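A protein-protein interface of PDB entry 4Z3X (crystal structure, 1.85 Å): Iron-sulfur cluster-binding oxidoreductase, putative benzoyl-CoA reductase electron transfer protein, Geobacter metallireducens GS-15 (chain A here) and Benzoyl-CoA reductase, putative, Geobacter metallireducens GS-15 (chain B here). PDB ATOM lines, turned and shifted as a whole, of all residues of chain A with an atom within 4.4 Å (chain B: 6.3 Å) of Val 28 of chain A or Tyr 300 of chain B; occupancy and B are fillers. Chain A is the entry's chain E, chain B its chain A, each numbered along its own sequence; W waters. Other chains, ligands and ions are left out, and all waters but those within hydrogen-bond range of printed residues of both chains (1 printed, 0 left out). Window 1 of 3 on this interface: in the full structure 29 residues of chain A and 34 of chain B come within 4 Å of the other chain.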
ATOM      1  N   CYS A  23     -16.840  24.556   6.633  1.00  0.00           N
ATOM      2  CA  CYS A  23     -15.495  24.940   6.135  1.00  0.00           C
ATOM      3  C   CYS A  23     -14.504  23.859   6.494  1.00  0.00           C
ATOM      4  O   CYS A  23     -13.470  23.686   5.834  1.00  0.00           O
ATOM      5  CB  CYS A  23     -15.041  26.265   6.721  1.00  0.00           C
ATOM      6  SG  CYS A  23     -14.746  26.310   8.457  1.00  0.00           S
ATOM      7  N   ARG A  24     -14.837  23.129   7.556  1.00  0.00           N
ATOM      8  CA  ARG A  24     -14.015  22.039   8.060  1.00  0.00           C
ATOM      9  C   ARG A  24     -12.711  22.526   8.663  1.00  0.00           C
ATOM     10  O   ARG A  24     -11.773  21.748   8.797  1.00  0.00           O
ATOM     11  CB  ARG A  24     -13.736  20.942   7.013  1.00  0.00           C
ATOM     12  CG  ARG A  24     -15.011  20.134   6.619  1.00  0.00           C
ATOM     13  CD  ARG A  24     -14.897  19.322   5.326  1.00  0.00           C
ATOM     14  NE  ARG A  24     -13.711  18.474   5.465  1.00  0.00           N
ATOM     15  CZ  ARG A  24     -12.910  18.064   4.489  1.00  0.00           C
ATOM     16  NH1 ARG A  24     -13.160  18.364   3.212  1.00  0.00           N
ATOM     17  NH2 ARG A  24     -11.847  17.342   4.832  1.00  0.00           N
ATOM     18  N   ALA A  25     -12.689  23.764   9.155  1.00  0.00           N
ATOM     19  CA  ALA A  25     -11.484  24.337   9.807  1.00  0.00           C
ATOM     20  C   ALA A  25     -11.152  23.576  11.110  1.00  0.00           C
ATOM     21  O   ALA A  25      -9.995  23.413  11.566  1.00  0.00           O
ATOM     22  CB  ALA A  25     -11.722  25.941  10.113  1.00  0.00           C
ATOM     23  N   CYS A  26     -12.204  23.121  11.754  1.00  0.00           N
ATOM     24  CA  CYS A  26     -12.116  22.327  12.953  1.00  0.00           C
ATOM     25  C   CYS A  26     -11.372  21.007  12.749  1.00  0.00           C
ATOM     26  O   CYS A  26     -10.483  20.641  13.566  1.00  0.00           O
ATOM     27  CB  CYS A  26     -13.547  22.121  13.471  1.00  0.00           C
ATOM     28  SG  CYS A  26     -14.842  21.576  12.256  1.00  0.00           S
ATOM     29  N   GLU A  27     -11.657  20.349  11.625  1.00  0.00           N
ATOM     30  CA  GLU A  27     -10.936  19.129  11.290  1.00  0.00           C
ATOM     31  C   GLU A  27      -9.494  19.450  11.025  1.00  0.00           C
ATOM     32  O   GLU A  27      -8.641  18.635  11.363  1.00  0.00           O
ATOM     33  CB  GLU A  27     -11.521  18.437  10.063  1.00  0.00           C
ATOM     34  CG  GLU A  27     -12.996  18.188  10.160  1.00  0.00           C
ATOM     35  CD  GLU A  27     -13.570  17.418   8.994  1.00  0.00           C
ATOM     36  OE1 GLU A  27     -12.874  17.110   8.002  1.00  0.00           O
ATOM     37  OE2 GLU A  27     -14.769  17.127   9.015  1.00  0.00           O
ATOM     38  N   VAL A  28      -9.203  20.612  10.381  1.00  0.00           N
ATOM     39  CA  VAL A  28      -7.836  20.876  10.087  1.00  0.00           C
ATOM     40  C   VAL A  28      -7.108  21.036  11.382  1.00  0.00           C
ATOM     41  O   VAL A  28      -6.072  20.401  11.629  1.00  0.00           O
ATOM     42  CB  VAL A  28      -7.647  22.180   9.240  1.00  0.00           C
ATOM     43  CG1 VAL A  28      -6.189  22.538   9.180  1.00  0.00           C
ATOM     44  CG2 VAL A  28      -8.242  22.033   7.832  1.00  0.00           C
ATOM     45  N   ILE A  29      -7.607  21.927  12.235  1.00  0.00           N
ATOM     46  CA  ILE A  29      -6.791  22.268  13.411  1.00  0.00           C
ATOM     47  C   ILE A  29      -6.681  21.062  14.402  1.00  0.00           C
ATOM     48  O   ILE A  29      -5.582  20.782  14.965  1.00  0.00           O
ATOM     49  CB  ILE A  29      -7.355  23.527  14.122  1.00  0.00           C
ATOM     50  CG1 ILE A  29      -6.361  24.083  15.141  1.00  0.00           C
ATOM     51  CG2 ILE A  29      -8.578  23.195  14.960  1.00  0.00           C
ATOM     52  CD1 ILE A  29      -4.978  24.244  14.581  1.00  0.00           C
ATOM     53  N   CYS A  30      -7.775  20.321  14.601  1.00  0.00           N
ATOM     54  CA  CYS A  30      -7.728  19.205  15.587  1.00  0.00           C
ATOM     55  C   CYS A  30      -6.700  18.146  15.140  1.00  0.00           C
ATOM     56  O   CYS A  30      -5.797  17.811  15.923  1.00  0.00           O
ATOM     57  CB  CYS A  30      -9.098  18.579  15.791  1.00  0.00           C
ATOM     58  SG  CYS A  30      -9.084  17.098  16.890  1.00  0.00           S
ATOM     59  N   SER A  31      -6.781  17.695  13.888  1.00  0.00           N
ATOM     60  CA  SER A  31      -5.738  16.794  13.368  1.00  0.00           C
ATOM     61  C   SER A  31      -4.313  17.360  13.469  1.00  0.00           C
ATOM     62  O   SER A  31      -3.399  16.628  13.870  1.00  0.00           O
ATOM     63  CB  SER A  31      -6.054  16.320  11.914  1.00  0.00           C
ATOM     64  OG  SER A  31      -5.990  17.334  10.829  1.00  0.00           O
ATOM     65  N   ALA A  32      -4.117  18.663  13.210  1.00  0.00           N
ATOM     66  CA  ALA A  32      -2.776  19.244  13.197  1.00  0.00           C
ATOM     67  C   ALA A  32      -2.229  19.239  14.602  1.00  0.00           C
ATOM     68  O   ALA A  32      -1.071  18.883  14.870  1.00  0.00           O
ATOM     69  CB  ALA A  32      -2.781  20.712  12.620  1.00  0.00           C
ATOM     70  N   ASN A  42      -1.158  17.658   9.080  1.00  0.00           N
ATOM     71  CA  ASN A  42      -2.590  17.582   9.387  1.00  0.00           C
ATOM     72  C   ASN A  42      -3.177  16.565   8.448  1.00  0.00           C
ATOM     73  O   ASN A  42      -2.554  16.191   7.452  1.00  0.00           O
ATOM     74  CB  ASN A  42      -3.298  18.926   9.258  1.00  0.00           C
ATOM     75  CG  ASN A  42      -3.677  19.278   7.856  1.00  0.00           C
ATOM     76  OD1 ASN A  42      -4.844  19.150   7.482  1.00  0.00           O
ATOM     77  ND2 ASN A  42      -2.723  19.855   7.075  1.00  0.00           N
ATOM     78  N   PRO A  44      -7.374  15.465   7.903  1.00  0.00           N
ATOM     79  CA  PRO A  44      -8.717  15.413   8.505  1.00  0.00           C
ATOM     80  C   PRO A  44      -9.253  13.995   8.880  1.00  0.00           C
ATOM     81  O   PRO A  44     -10.141  13.933   9.775  1.00  0.00           O
ATOM     82  CB  PRO A  44      -9.614  16.044   7.437  1.00  0.00           C
ATOM     83  CG  PRO A  44      -8.659  17.029   6.687  1.00  0.00           C
ATOM     84  CD  PRO A  44      -7.352  16.229   6.643  1.00  0.00           C
ATOM     85  N   GLY B  69      -3.738  22.008   1.402  1.00  0.00           N
ATOM     86  CA  GLY B  69      -3.656  20.855   2.274  1.00  0.00           C
ATOM     87  C   GLY B  69      -2.859  21.143   3.532  1.00  0.00           C
ATOM     88  O   GLY B  69      -2.720  20.263   4.374  1.00  0.00           O
ATOM     89  N   THR B  70      -2.332  22.364   3.670  1.00  0.00           N
ATOM     90  CA  THR B  70      -1.673  22.759   4.918  1.00  0.00           C
ATOM     91  C   THR B  70      -2.715  23.497   5.758  1.00  0.00           C
ATOM     92  O   THR B  70      -3.802  23.772   5.269  1.00  0.00           O
ATOM     93  CB  THR B  70      -0.446  23.703   4.697  1.00  0.00           C
ATOM     94  OG1 THR B  70      -0.902  24.964   4.205  1.00  0.00           O
ATOM     95  CG2 THR B  70       0.599  23.121   3.726  1.00  0.00           C
ATOM     96  N   PRO B  71      -2.390  23.876   7.005  1.00  0.00           N
ATOM     97  CA  PRO B  71      -3.461  24.574   7.757  1.00  0.00           C
ATOM     98  C   PRO B  71      -3.679  26.047   7.378  1.00  0.00           C
ATOM     99  O   PRO B  71      -4.473  26.716   8.063  1.00  0.00           O
ATOM    100  CB  PRO B  71      -2.998  24.490   9.221  1.00  0.00           C
ATOM    101  CG  PRO B  71      -1.965  23.436   9.277  1.00  0.00           C
ATOM    102  CD  PRO B  71      -1.278  23.475   7.883  1.00  0.00           C
ATOM    103  N   ALA B  72      -3.024  26.558   6.324  1.00  0.00           N
ATOM    104  CA  ALA B  72      -3.220  27.968   5.973  1.00  0.00           C
ATOM    105  C   ALA B  72      -4.655  28.308   5.541  1.00  0.00           C
ATOM    106  O   ALA B  72      -5.184  27.753   4.571  1.00  0.00           O
ATOM    107  CB  ALA B  72      -2.242  28.382   4.889  1.00  0.00           C
ATOM    108  N   THR B  73      -5.273  29.255   6.256  1.00  0.00           N
ATOM    109  CA  THR B  73      -6.654  29.666   5.990  1.00  0.00           C
ATOM    110  C   THR B  73      -6.919  29.977   4.524  1.00  0.00           C
ATOM    111  O   THR B  73      -6.143  30.716   3.879  1.00  0.00           O
ATOM    112  CB  THR B  73      -7.008  30.912   6.851  1.00  0.00           C
ATOM    113  OG1 THR B  73      -6.635  30.640   8.198  1.00  0.00           O
ATOM    114  CG2 THR B  73      -8.504  31.229   6.795  1.00  0.00           C
ATOM    115  N   GLY B  74      -8.001  29.413   3.986  1.00  0.00           N
ATOM    116  CA  GLY B  74      -8.390  29.705   2.623  1.00  0.00           C
ATOM    117  C   GLY B  74      -7.389  29.271   1.529  1.00  0.00           C
ATOM    118  O   GLY B  74      -7.548  29.662   0.373  1.00  0.00           O
ATOM    119  N   CYS B  75      -6.376  28.459   1.846  1.00  0.00           N
ATOM    120  CA  CYS B  75      -5.455  28.004   0.811  1.00  0.00           C
ATOM    121  C   CYS B  75      -5.944  26.667   0.214  1.00  0.00           C
ATOM    122  O   CYS B  75      -5.654  25.590   0.727  1.00  0.00           O
ATOM    123  CB  CYS B  75      -4.021  27.888   1.369  1.00  0.00           C
ATOM    124  SG  CYS B  75      -2.791  27.595   0.053  1.00  0.00           S
ATOM    125  N   ASN B  76      -6.745  26.737  -0.835  1.00  0.00           N
ATOM    126  CA  ASN B  76      -7.487  25.564  -1.281  1.00  0.00           C
ATOM    127  C   ASN B  76      -7.713  25.536  -2.794  1.00  0.00           C
ATOM    128  O   ASN B  76      -8.577  24.775  -3.279  1.00  0.00           O
ATOM    129  CB  ASN B  76      -8.843  25.552  -0.529  1.00  0.00           C
ATOM    130  CG  ASN B  76      -9.547  26.914  -0.639  1.00  0.00           C
ATOM    131  OD1 ASN B  76      -9.421  27.542  -1.652  1.00  0.00           O
ATOM    132  ND2 ASN B  76     -10.235  27.377   0.416  1.00  0.00           N
ATOM    133  N   GLY B  96     -11.937  27.015  -6.399  1.00  0.00           N
ATOM    134  CA  GLY B  96     -11.839  26.920  -4.955  1.00  0.00           C
ATOM    135  C   GLY B  96     -12.461  25.636  -4.389  1.00  0.00           C
ATOM    136  O   GLY B  96     -12.361  24.577  -4.987  1.00  0.00           O
ATOM    137  N   GLY B  97     -13.079  25.724  -3.222  1.00  0.00           N
ATOM    138  CA  GLY B  97     -13.750  24.554  -2.635  1.00  0.00           C
ATOM    139  C   GLY B  97     -12.820  23.618  -1.897  1.00  0.00           C
ATOM    140  O   GLY B  97     -12.038  24.040  -1.011  1.00  0.00           O
ATOM    141  N   PHE B  98     -12.883  22.348  -2.254  1.00  0.00           N
ATOM    142  CA  PHE B  98     -12.362  21.265  -1.419  1.00  0.00           C
ATOM    143  C   PHE B  98     -11.499  20.267  -2.225  1.00  0.00           C
ATOM    144  O   PHE B  98     -10.895  19.329  -1.666  1.00  0.00           O
ATOM    145  CB  PHE B  98     -13.530  20.530  -0.701  1.00  0.00           C
ATOM    146  CG  PHE B  98     -14.324  21.430   0.213  1.00  0.00           C
ATOM    147  CD1 PHE B  98     -15.300  22.296  -0.285  1.00  0.00           C
ATOM    148  CD2 PHE B  98     -14.058  21.448   1.546  1.00  0.00           C
ATOM    149  CE1 PHE B  98     -16.035  23.149   0.590  1.00  0.00           C
ATOM    150  CE2 PHE B  98     -14.796  22.326   2.466  1.00  0.00           C
ATOM    151  CZ  PHE B  98     -15.779  23.138   1.968  1.00  0.00           C
ATOM    152  N   PRO B 101      -7.215  20.546  -1.861  1.00  0.00           N
ATOM    153  CA  PRO B 101      -6.740  19.924  -0.639  1.00  0.00           C
ATOM    154  C   PRO B 101      -6.921  18.364  -0.626  1.00  0.00           C
ATOM    155  O   PRO B 101      -6.055  17.622  -0.113  1.00  0.00           O
ATOM    156  CB  PRO B 101      -7.613  20.586   0.436  1.00  0.00           C
ATOM    157  CG  PRO B 101      -7.922  21.968  -0.150  1.00  0.00           C
ATOM    158  CD  PRO B 101      -8.166  21.645  -1.598  1.00  0.00           C
ATOM    159  N   TYR B 105      -4.066  15.379   0.052  1.00  0.00           N
ATOM    160  CA  TYR B 105      -4.205  14.343   1.097  1.00  0.00           C
ATOM    161  C   TYR B 105      -4.159  12.964   0.424  1.00  0.00           C
ATOM    162  O   TYR B 105      -3.931  11.944   1.085  1.00  0.00           O
ATOM    163  CB  TYR B 105      -5.497  14.506   1.917  1.00  0.00           C
ATOM    164  CG  TYR B 105      -5.583  15.757   2.788  1.00  0.00           C
ATOM    165  CD1 TYR B 105      -4.563  16.090   3.680  1.00  0.00           C
ATOM    166  CD2 TYR B 105      -6.655  16.626   2.655  1.00  0.00           C
ATOM    167  CE1 TYR B 105      -4.634  17.263   4.474  1.00  0.00           C
ATOM    168  CE2 TYR B 105      -6.736  17.800   3.432  1.00  0.00           C
ATOM    169  CZ  TYR B 105      -5.735  18.097   4.336  1.00  0.00           C
ATOM    170  OH  TYR B 105      -5.851  19.250   5.075  1.00  0.00           O
ATOM    171  N   SER B 298     -18.689  28.245   3.083  1.00  0.00           N
ATOM    172  CA  SER B 298     -17.305  28.553   2.792  1.00  0.00           C
ATOM    173  C   SER B 298     -16.621  27.514   1.857  1.00  0.00           C
ATOM    174  O   SER B 298     -17.076  26.374   1.720  1.00  0.00           O
ATOM    175  CB  SER B 298     -16.505  28.627   4.094  1.00  0.00           C
ATOM    176  OG  SER B 298     -16.914  29.664   4.985  1.00  0.00           O
ATOM    177  N   CYS B 299     -15.505  27.904   1.246  1.00  0.00           N
ATOM    178  CA  CYS B 299     -14.537  26.883   0.786  1.00  0.00           C
ATOM    179  C   CYS B 299     -13.821  26.229   1.980  1.00  0.00           C
ATOM    180  O   CYS B 299     -14.143  26.533   3.150  1.00  0.00           O
ATOM    181  CB  CYS B 299     -13.500  27.547  -0.159  1.00  0.00           C
ATOM    182  SG  CYS B 299     -14.316  28.398  -1.435  1.00  0.00           S
ATOM    183  N   TYR B 300     -12.882  25.336   1.689  1.00  0.00           N
ATOM    184  CA  TYR B 300     -12.108  24.602   2.695  1.00  0.00           C
ATOM    185  C   TYR B 300     -11.300  25.498   3.576  1.00  0.00           C
ATOM    186  O   TYR B 300     -10.595  26.347   3.078  1.00  0.00           O
ATOM    187  CB  TYR B 300     -11.162  23.627   2.038  1.00  0.00           C
ATOM    188  CG  TYR B 300     -10.411  22.717   2.980  1.00  0.00           C
ATOM    189  CD1 TYR B 300     -11.111  21.818   3.814  1.00  0.00           C
ATOM    190  CD2 TYR B 300      -9.007  22.704   3.028  1.00  0.00           C
ATOM    191  CE1 TYR B 300     -10.453  20.958   4.654  1.00  0.00           C
ATOM    192  CE2 TYR B 300      -8.316  21.798   3.875  1.00  0.00           C
ATOM    193  CZ  TYR B 300      -9.061  20.936   4.682  1.00  0.00           C
ATOM    194  OH  TYR B 300      -8.444  20.010   5.514  1.00  0.00           O
ATOM    195  N   ASN B 301     -11.425  25.304   4.890  1.00  0.00           N
ATOM    196  CA  ASN B 301     -10.653  26.009   5.903  1.00  0.00           C
ATOM    197  C   ASN B 301     -10.703  27.569   5.727  1.00  0.00           C
ATOM    198  O   ASN B 301      -9.694  28.251   5.832  1.00  0.00           O
ATOM    199  CB  ASN B 301      -9.206  25.491   5.859  1.00  0.00           C
ATOM    200  CG  ASN B 301      -8.387  25.943   7.053  1.00  0.00           C
ATOM    201  OD1 ASN B 301      -8.924  26.170   8.145  1.00  0.00           O
ATOM    202  ND2 ASN B 301      -7.070  26.091   6.849  1.00  0.00           N
ATOM    203  N   CYS B 302     -11.908  28.101   5.557  1.00  0.00           N
ATOM    204  CA  CYS B 302     -12.115  29.532   5.550  1.00  0.00           C
ATOM    205  C   CYS B 302     -13.395  30.030   6.234  1.00  0.00           C
ATOM    206  O   CYS B 302     -14.494  29.487   5.978  1.00  0.00           O
ATOM    207  CB  CYS B 302     -12.123  30.012   4.084  1.00  0.00           C
ATOM    208  SG  CYS B 302     -12.172  31.795   3.930  1.00  0.00           S
HETATM  209  O   HOH W   1     -11.206  18.113   1.123  1.00  0.00           O
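The side-chain hydroxyl (OH) of Tyr 105 of chain B is in hydrogen-bond range of the side-chain amide oxygen (OD1) of Asn 42 of chain A (2.6 Å).
ND2 of Asn 42 of chain A sits at hydrogen-bond distance from O of Gly 69 of chain B (2.7 Å).
The backbone NH (N) of Asn 301 of chain B sits at hydrogen-bond distance from the backbone carbonyl oxygen (O) of Cys 23 of chain A, 2.8 Å away.
Hydrophobic or aromatic side chains of chain B within 4 Å of the printed part of chain A: Pro 71, Phe 98, Tyr 105 and Tyr 300.
Hydrophobic or aromatic side chains of chain A within 4 Å of the printed part of chain B: Ala 25, Val 28 and Pro 44.
Water W1 lies within hydrogen-bond range of the guanidinium group of Arg 24 of chain A (2.9 Å) and the backbone carbonyl oxygen of Phe 98 of chain B (3.1 Å).
Among the printed residues, pairs that only touch across the chains: Val 28 of chain A with Tyr 300 of chain B (3.1 Å), Pro 44 of chain A with Tyr 300 of chain B (3.2 Å), Cys 23 of chain A with Cys 302 of chain B (3.4 Å), Pro 44 of chain A with Tyr 105 of chain B (3.4 Å), Ala 25 of chain A with Asn 301 of chain B (3.4 Å), Cys 23 of chain A with Tyr 300 of chain B (3.5 Å), Arg 24 of chain A with Phe 98 of chain B (3.6 Å), Cys 23 of chain A with Cys 299 of chain B (3.6 Å), Val 28 of chain A with Pro 71 of chain B (3.7 Å), Asn 42 of chain A with Thr 70 of chain B (3.8 Å), Arg 24 of chain A with Tyr 300 of chain B (3.8 Å), Cys 23 of chain A with Ser 298 of chain B (3.8 Å), Cys 23 of chain A with Phe 98 of chain B (3.9 Å), Asn 42 of chain A with Pro 71 of chain B (3.98 Å) and Val 28 of chain A with Asn 301 of chain B (3.99 Å).
Printed residues of chain B within 4 Å of Val 28 of chain A: Pro 71, Tyr 300 and Asn 301.
Of the printed residues of chain A, Thr 70 of chain B touches Asn 42 (3.8 Å).
Printed residues of chain B within 4 Å of Ala 25 of chain A: Asn 301.
Glu 27 of chain A touches none of the printed residues of chain B.
Gly 97 of chain B touches none of the printed residues of chain A.
The nearest printed residue of chain B that does not touch Val 28 of chain A is Tyr 105 of chain B (4.6 Å).
The side-chain hydroxyl (OG) of Ser 298 of chain B sits at hydrogen-bond distance from the backbone carbonyl oxygen (O) of Cys 302 of chain B.
The backbone NH (N) of Ala 72 of chain B lies close to the side-chain hydroxyl (OG1) of Thr 70 of chain B, 3.4 Å away.
The guanidinium group (NE) of Arg 24 of chain A lies within salt-bridge range of the side-chain carboxylate (OE1) of Glu 27 of chain A, 3.0 Å away.
The backbone carbonyl oxygen of Gly 69 of chain B lies within hydrogen-bond range of the side-chain hydroxyl of Tyr 105 of chain B (3.4 Å).
The side-chain hydroxyl of Tyr 105 of chain B lies within hydrogen-bond range of the side-chain hydroxyl of Tyr 300 of chain B (2.7 Å).
The backbone NH of Gly 97 of chain B lies close to the side-chain sulfur of Cys 299 of chain B.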
